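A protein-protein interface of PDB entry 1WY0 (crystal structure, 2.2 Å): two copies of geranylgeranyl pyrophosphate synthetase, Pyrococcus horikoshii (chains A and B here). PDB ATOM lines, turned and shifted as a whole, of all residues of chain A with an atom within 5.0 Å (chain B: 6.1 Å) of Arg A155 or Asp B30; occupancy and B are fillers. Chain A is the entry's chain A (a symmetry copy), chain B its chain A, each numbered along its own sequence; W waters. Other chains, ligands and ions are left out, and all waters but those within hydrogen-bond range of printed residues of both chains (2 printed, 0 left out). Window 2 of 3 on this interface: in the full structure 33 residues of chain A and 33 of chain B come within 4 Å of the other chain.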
ATOM      1  N   GLU A 151       2.179 -20.188  -3.927  1.00  0.00           N
ATOM      2  CA  GLU A 151       2.763 -19.578  -2.734  1.00  0.00           C
ATOM      3  C   GLU A 151       1.992 -18.343  -2.305  1.00  0.00           C
ATOM      4  O   GLU A 151       1.759 -18.142  -1.123  1.00  0.00           O
ATOM      5  CB  GLU A 151       4.231 -19.229  -2.983  1.00  0.00           C
ATOM      6  CG  GLU A 151       5.158 -20.431  -2.879  1.00  0.00           C
ATOM      7  CD  GLU A 151       6.523 -20.152  -3.448  1.00  0.00           C
ATOM      8  OE1 GLU A 151       6.771 -18.986  -3.834  1.00  0.00           O
ATOM      9  OE2 GLU A 151       7.352 -21.094  -3.512  1.00  0.00           O
ATOM     10  N   GLY A 152       1.579 -17.530  -3.272  1.00  0.00           N
ATOM     11  CA  GLY A 152       0.819 -16.335  -2.957  1.00  0.00           C
ATOM     12  C   GLY A 152      -0.548 -16.682  -2.410  1.00  0.00           C
ATOM     13  O   GLY A 152      -1.058 -16.013  -1.510  1.00  0.00           O
ATOM     14  N   GLN A 153      -1.164 -17.724  -2.955  1.00  0.00           N
ATOM     15  CA  GLN A 153      -2.468 -18.132  -2.479  1.00  0.00           C
ATOM     16  C   GLN A 153      -2.333 -18.758  -1.079  1.00  0.00           C
ATOM     17  O   GLN A 153      -3.212 -18.597  -0.239  1.00  0.00           O
ATOM     18  CB  GLN A 153      -3.106 -19.115  -3.469  1.00  0.00           C
ATOM     19  CG  GLN A 153      -4.446 -19.682  -3.022  1.00  0.00           C
ATOM     20  CD  GLN A 153      -5.503 -18.617  -2.763  1.00  0.00           C
ATOM     21  OE1 GLN A 153      -5.227 -17.420  -2.861  1.00  0.00           O
ATOM     22  NE2 GLN A 153      -6.717 -19.048  -2.428  1.00  0.00           N
ATOM     23  N   ALA A 154      -1.230 -19.457  -0.828  1.00  0.00           N
ATOM     24  CA  ALA A 154      -0.995 -20.071   0.480  1.00  0.00           C
ATOM     25  C   ALA A 154      -0.898 -18.976   1.548  1.00  0.00           C
ATOM     26  O   ALA A 154      -1.528 -19.054   2.600  1.00  0.00           O
ATOM     27  CB  ALA A 154       0.287 -20.880   0.462  1.00  0.00           C
ATOM     28  N   ARG A 155      -0.095 -17.956   1.280  1.00  0.00           N
ATOM     29  CA  ARG A 155       0.043 -16.860   2.230  1.00  0.00           C
ATOM     30  C   ARG A 155      -1.308 -16.198   2.434  1.00  0.00           C
ATOM     31  O   ARG A 155      -1.616 -15.721   3.521  1.00  0.00           O
ATOM     32  CB  ARG A 155       1.033 -15.817   1.716  1.00  0.00           C
ATOM     33  CG  ARG A 155       2.418 -16.341   1.464  1.00  0.00           C
ATOM     34  CD  ARG A 155       3.376 -15.180   1.341  1.00  0.00           C
ATOM     35  NE  ARG A 155       4.228 -15.309   0.174  1.00  0.00           N
ATOM     36  CZ  ARG A 155       5.459 -15.808   0.184  1.00  0.00           C
ATOM     37  NH1 ARG A 155       6.007 -16.234   1.312  1.00  0.00           N
ATOM     38  NH2 ARG A 155       6.141 -15.874  -0.949  1.00  0.00           N
ATOM     39  N   ASP A 156      -2.121 -16.176   1.384  1.00  0.00           N
ATOM     40  CA  ASP A 156      -3.436 -15.561   1.487  1.00  0.00           C
ATOM     41  C   ASP A 156      -4.319 -16.381   2.420  1.00  0.00           C
ATOM     42  O   ASP A 156      -5.145 -15.825   3.147  1.00  0.00           O
ATOM     43  CB  ASP A 156      -4.086 -15.418   0.106  1.00  0.00           C
ATOM     44  CG  ASP A 156      -5.194 -14.373   0.094  1.00  0.00           C
ATOM     45  OD1 ASP A 156      -5.080 -13.368   0.841  1.00  0.00           O
ATOM     46  OD2 ASP A 156      -6.171 -14.533  -0.664  1.00  0.00           O
ATOM     47  N   LEU A 157      -4.137 -17.701   2.416  1.00  0.00           N
ATOM     48  CA  LEU A 157      -4.921 -18.555   3.305  1.00  0.00           C
ATOM     49  C   LEU A 157      -4.493 -18.329   4.757  1.00  0.00           C
ATOM     50  O   LEU A 157      -5.332 -18.245   5.641  1.00  0.00           O
ATOM     51  CB  LEU A 157      -4.738 -20.034   2.961  1.00  0.00           C
ATOM     52  CG  LEU A 157      -5.428 -20.568   1.712  1.00  0.00           C
ATOM     53  CD1 LEU A 157      -5.115 -22.051   1.555  1.00  0.00           C
ATOM     54  CD2 LEU A 157      -6.920 -20.343   1.826  1.00  0.00           C
ATOM     55  N   GLU A 158      -3.191 -18.230   4.998  1.00  0.00           N
ATOM     56  CA  GLU A 158      -2.691 -18.016   6.359  1.00  0.00           C
ATOM     57  C   GLU A 158      -3.275 -16.754   6.990  1.00  0.00           C
ATOM     58  O   GLU A 158      -3.509 -16.713   8.192  1.00  0.00           O
ATOM     59  CB  GLU A 158      -1.157 -17.942   6.370  1.00  0.00           C
ATOM     60  CG  GLU A 158      -0.465 -19.288   6.107  1.00  0.00           C
ATOM     61  CD  GLU A 158      -0.418 -20.201   7.329  1.00  0.00           C
ATOM     62  OE1 GLU A 158       0.559 -20.106   8.106  1.00  0.00           O
ATOM     63  OE2 GLU A 158      -1.355 -21.011   7.519  1.00  0.00           O
ATOM     64  N   PHE A 159      -3.513 -15.726   6.180  1.00  0.00           N
ATOM     65  CA  PHE A 159      -4.085 -14.473   6.671  1.00  0.00           C
ATOM     66  C   PHE A 159      -5.354 -14.721   7.488  1.00  0.00           C
ATOM     67  O   PHE A 159      -5.665 -14.023   8.443  1.00  0.00           O
ATOM     68  CB  PHE A 159      -4.428 -13.590   5.470  1.00  0.00           C
ATOM     69  CG  PHE A 159      -3.195 -12.952   4.898  1.00  0.00           C
ATOM     70  CD1 PHE A 159      -2.019 -12.909   5.642  1.00  0.00           C
ATOM     71  CD2 PHE A 159      -3.253 -12.361   3.648  1.00  0.00           C
ATOM     72  CE1 PHE A 159      -0.902 -12.267   5.122  1.00  0.00           C
ATOM     73  CE2 PHE A 159      -2.132 -11.722   3.135  1.00  0.00           C
ATOM     74  CZ  PHE A 159      -0.951 -11.672   3.866  1.00  0.00           C
ATOM     75  N   GLU A 172       3.574  -8.938  -0.477  1.00  0.00           N
ATOM     76  CA  GLU A 172       4.339 -10.128  -0.817  1.00  0.00           C
ATOM     77  C   GLU A 172       3.376 -11.203  -1.336  1.00  0.00           C
ATOM     78  O   GLU A 172       3.719 -12.002  -2.203  1.00  0.00           O
ATOM     79  CB  GLU A 172       5.102 -10.631   0.410  1.00  0.00           C
ATOM     80  CG  GLU A 172       5.885 -11.901   0.163  1.00  0.00           C
ATOM     81  CD  GLU A 172       6.548 -12.438   1.414  1.00  0.00           C
ATOM     82  OE1 GLU A 172       5.935 -12.323   2.493  1.00  0.00           O
ATOM     83  OE2 GLU A 172       7.670 -12.992   1.317  1.00  0.00           O
ATOM     84  N   MET A 173       2.156 -11.178  -0.812  1.00  0.00           N
ATOM     85  CA  MET A 173       1.117 -12.123  -1.182  1.00  0.00           C
ATOM     86  C   MET A 173       0.551 -11.803  -2.565  1.00  0.00           C
ATOM     87  O   MET A 173       0.530 -12.662  -3.457  1.00  0.00           O
ATOM     88  CB  MET A 173       0.012 -12.078  -0.122  1.00  0.00           C
ATOM     89  CG  MET A 173      -1.225 -12.943  -0.402  1.00  0.00           C
ATOM     90  SD  MET A 173      -2.370 -12.270  -1.638  1.00  0.00           S
ATOM     91  CE  MET A 173      -3.297 -11.054  -0.679  1.00  0.00           C
ATOM     92  N   GLU B  28      12.156 -26.984   2.971  1.00  0.00           N
ATOM     93  CA  GLU B  28      11.425 -26.267   4.012  1.00  0.00           C
ATOM     94  C   GLU B  28      11.621 -24.752   3.893  1.00  0.00           C
ATOM     95  O   GLU B  28      12.478 -24.147   4.525  1.00  0.00           O
ATOM     96  CB  GLU B  28      11.933 -26.753   5.371  1.00  0.00           C
ATOM     97  CG  GLU B  28      12.243 -28.252   5.379  1.00  0.00           C
ATOM     98  CD  GLU B  28      12.934 -28.614   6.674  1.00  0.00           C
ATOM     99  OE1 GLU B  28      14.137 -28.417   6.772  1.00  0.00           O
ATOM    100  OE2 GLU B  28      12.259 -29.104   7.579  1.00  0.00           O
ATOM    101  N   LYS B  29      10.808 -24.140   3.012  1.00  0.00           N
ATOM    102  CA  LYS B  29      10.933 -22.705   2.783  1.00  0.00           C
ATOM    103  C   LYS B  29       9.568 -22.012   2.789  1.00  0.00           C
ATOM    104  O   LYS B  29       8.517 -22.635   2.872  1.00  0.00           O
ATOM    105  CB  LYS B  29      11.618 -22.493   1.433  1.00  0.00           C
ATOM    106  CG  LYS B  29      10.845 -23.142   0.283  1.00  0.00           C
ATOM    107  CD  LYS B  29      10.900 -22.308  -0.997  1.00  0.00           C
ATOM    108  CE  LYS B  29      11.545 -23.066  -2.162  1.00  0.00           C
ATOM    109  NZ  LYS B  29      11.233 -22.394  -3.421  1.00  0.00           N
ATOM    110  N   ASP B  30       9.614 -20.668   2.736  1.00  0.00           N
ATOM    111  CA  ASP B  30       8.373 -19.901   2.770  1.00  0.00           C
ATOM    112  C   ASP B  30       7.574 -20.055   1.473  1.00  0.00           C
ATOM    113  O   ASP B  30       8.092 -19.967   0.369  1.00  0.00           O
ATOM    114  CB  ASP B  30       8.728 -18.429   2.988  1.00  0.00           C
ATOM    115  CG  ASP B  30       8.538 -18.079   4.457  1.00  0.00           C
ATOM    116  OD1 ASP B  30       9.422 -18.417   5.243  1.00  0.00           O
ATOM    117  OD2 ASP B  30       7.523 -17.476   4.795  1.00  0.00           O
ATOM    118  N   PRO B  31       6.267 -20.336   1.644  1.00  0.00           N
ATOM    119  CA  PRO B  31       5.643 -20.564   2.942  1.00  0.00           C
ATOM    120  C   PRO B  31       5.768 -22.026   3.399  1.00  0.00           C
ATOM    121  O   PRO B  31       5.573 -22.972   2.647  1.00  0.00           O
ATOM    122  CB  PRO B  31       4.173 -20.169   2.845  1.00  0.00           C
ATOM    123  CG  PRO B  31       3.892 -19.725   1.415  1.00  0.00           C
ATOM    124  CD  PRO B  31       5.211 -20.222   0.654  1.00  0.00           C
ATOM    125  N   ARG B  32       6.134 -22.185   4.689  1.00  0.00           N
ATOM    126  CA  ARG B  32       6.431 -23.513   5.226  1.00  0.00           C
ATOM    127  C   ARG B  32       5.182 -24.404   5.310  1.00  0.00           C
ATOM    128  O   ARG B  32       5.185 -25.568   4.924  1.00  0.00           O
ATOM    129  CB  ARG B  32       7.026 -23.339   6.625  1.00  0.00           C
ATOM    130  CG  ARG B  32       8.552 -23.372   6.630  1.00  0.00           C
ATOM    131  CD  ARG B  32       9.122 -22.659   7.857  1.00  0.00           C
ATOM    132  NE  ARG B  32      10.586 -22.729   7.860  1.00  0.00           N
ATOM    133  CZ  ARG B  32      11.247 -21.651   7.409  1.00  0.00           C
ATOM    134  NH1 ARG B  32      10.576 -20.591   6.994  1.00  0.00           N
ATOM    135  NH2 ARG B  32      12.579 -21.643   7.425  1.00  0.00           N
ATOM    136  N   TYR B  35       4.794 -25.865   2.274  1.00  0.00           N
ATOM    137  CA  TYR B  35       5.851 -26.769   1.824  1.00  0.00           C
ATOM    138  C   TYR B  35       5.963 -28.019   2.708  1.00  0.00           C
ATOM    139  O   TYR B  35       6.457 -29.060   2.297  1.00  0.00           O
ATOM    140  CB  TYR B  35       7.174 -26.002   1.838  1.00  0.00           C
ATOM    141  CG  TYR B  35       7.422 -25.400   0.501  1.00  0.00           C
ATOM    142  CD1 TYR B  35       8.084 -26.136  -0.479  1.00  0.00           C
ATOM    143  CD2 TYR B  35       6.991 -24.104   0.217  1.00  0.00           C
ATOM    144  CE1 TYR B  35       8.304 -25.586  -1.733  1.00  0.00           C
ATOM    145  CE2 TYR B  35       7.219 -23.551  -1.034  1.00  0.00           C
ATOM    146  CZ  TYR B  35       7.877 -24.285  -2.004  1.00  0.00           C
ATOM    147  OH  TYR B  35       8.099 -23.744  -3.256  1.00  0.00           O
ATOM    148  N   MET B 109      -5.651 -25.900   2.087  1.00  0.00           N
ATOM    149  CA  MET B 109      -4.201 -26.001   2.023  1.00  0.00           C
ATOM    150  C   MET B 109      -3.782 -27.318   1.352  1.00  0.00           C
ATOM    151  O   MET B 109      -2.733 -27.389   0.709  1.00  0.00           O
ATOM    152  CB  MET B 109      -3.592 -25.896   3.423  1.00  0.00           C
ATOM    153  CG  MET B 109      -2.057 -25.786   3.422  1.00  0.00           C
ATOM    154  SD  MET B 109      -1.463 -24.325   2.508  1.00  0.00           S
ATOM    155  CE  MET B 109      -2.159 -22.977   3.552  1.00  0.00           C
ATOM    156  N   LEU B 112      -3.988 -26.765  -2.377  1.00  0.00           N
ATOM    157  CA  LEU B 112      -2.788 -26.025  -2.761  1.00  0.00           C
ATOM    158  C   LEU B 112      -1.513 -26.868  -2.727  1.00  0.00           C
ATOM    159  O   LEU B 112      -0.650 -26.685  -3.573  1.00  0.00           O
ATOM    160  CB  LEU B 112      -2.588 -24.805  -1.865  1.00  0.00           C
ATOM    161  CG  LEU B 112      -3.452 -23.598  -2.220  1.00  0.00           C
ATOM    162  CD1 LEU B 112      -3.047 -22.450  -1.340  1.00  0.00           C
ATOM    163  CD2 LEU B 112      -3.276 -23.225  -3.716  1.00  0.00           C
HETATM  164  O   HOH W   1       5.235 -16.230   4.255  1.00  0.00           O
HETATM  165  O   HOH W   2       9.596 -22.351  -5.392  1.00  0.00           O
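Water W2 lies within hydrogen-bond range of the side-chain amino group of Lys B29 (2.6 Å), the side-chain hydroxyl of Tyr B35 (3.0 Å) and the side-chain carboxylate of Glu A151 (3.2 Å).
Water W1 lies within hydrogen-bond range of the side-chain carboxylate (OD2) of Asp B30 (2.7 Å) and the guanidinium group (NH1) of Arg A155 (3.0 Å).
The side-chain amino group (NZ) of Lys B29 lies within hydrogen-bond range of the side-chain hydroxyl (OH) of Tyr B35 (3.4 Å).
NH1 of Arg A155 lies within salt-bridge range of OE2 of Glu A172.
The side-chain carboxylate (OD1) of Asp B30 is in salt-bridge range of the guanidinium group (NH1) of Arg B32, at 3.0 Å.
Of the printed residues of chain B, Gln A153 touches Leu B112 (3.5 Å).
Of the printed residues of chain B, Ala A154 touches Pro B31 and Leu B112.
Of chain B, only Asp B30 and Pro B31 come within 4 Å of Arg A155.
Asp A156 touches none of the printed residues of chain B.
Of the printed residues of chain B, Leu A157 touches Met B109 (3.7 Å) and Leu B112 (3.6 Å).
Asp B30 touches just one residue of chain A: Arg A155 (3.9 Å).
Of the printed residues of chain A, Tyr B35 touches Glu A151.
Printed residues of chain A within 4 Å of Leu B112: Gln A153, Ala A154 and Leu A157.
The nearest residue of chain B that does not touch Arg A155 is Met B109 (5.9 Å).
The nearest residue of chain A that does not touch Asp B30 is Glu A151 (4.1 Å).
No position is printed for both chains.
The guanidinium group of Arg A155 lies within salt-bridge range of the side-chain carboxylate of Asp B30 (3.997 Å).
OE2 of Glu A151 lies within hydrogen-bond range of OH of Tyr B35 (2.8 Å).
Of the 11 printed residues of chain A, 5 touch a printed residue of chain B.
Hydrophobic or aromatic side chains of chain A within 4 Å of the printed part of chain B: Ala A154 and Leu A157.
Along chain B the printed residues that touch a printed residue of chain A span positions 30 to 112.
Among the printed residues, 9 pairs touch across the chains.
Among the printed residues, Asp or Glu carboxylates within 4 Å of a Lys or Arg side-chain nitrogen of the other chain: Arg A155 with Asp B30.
Among the printed residues, merely in contact across the chains: Glu A151 with Pro B31, Gln A153 with Leu B112, Ala A154 with Pro B31, Ala A154 with Leu B112, Arg A155 with Pro B31, Leu A157 with Met B109 and Leu A157 with Leu B112.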
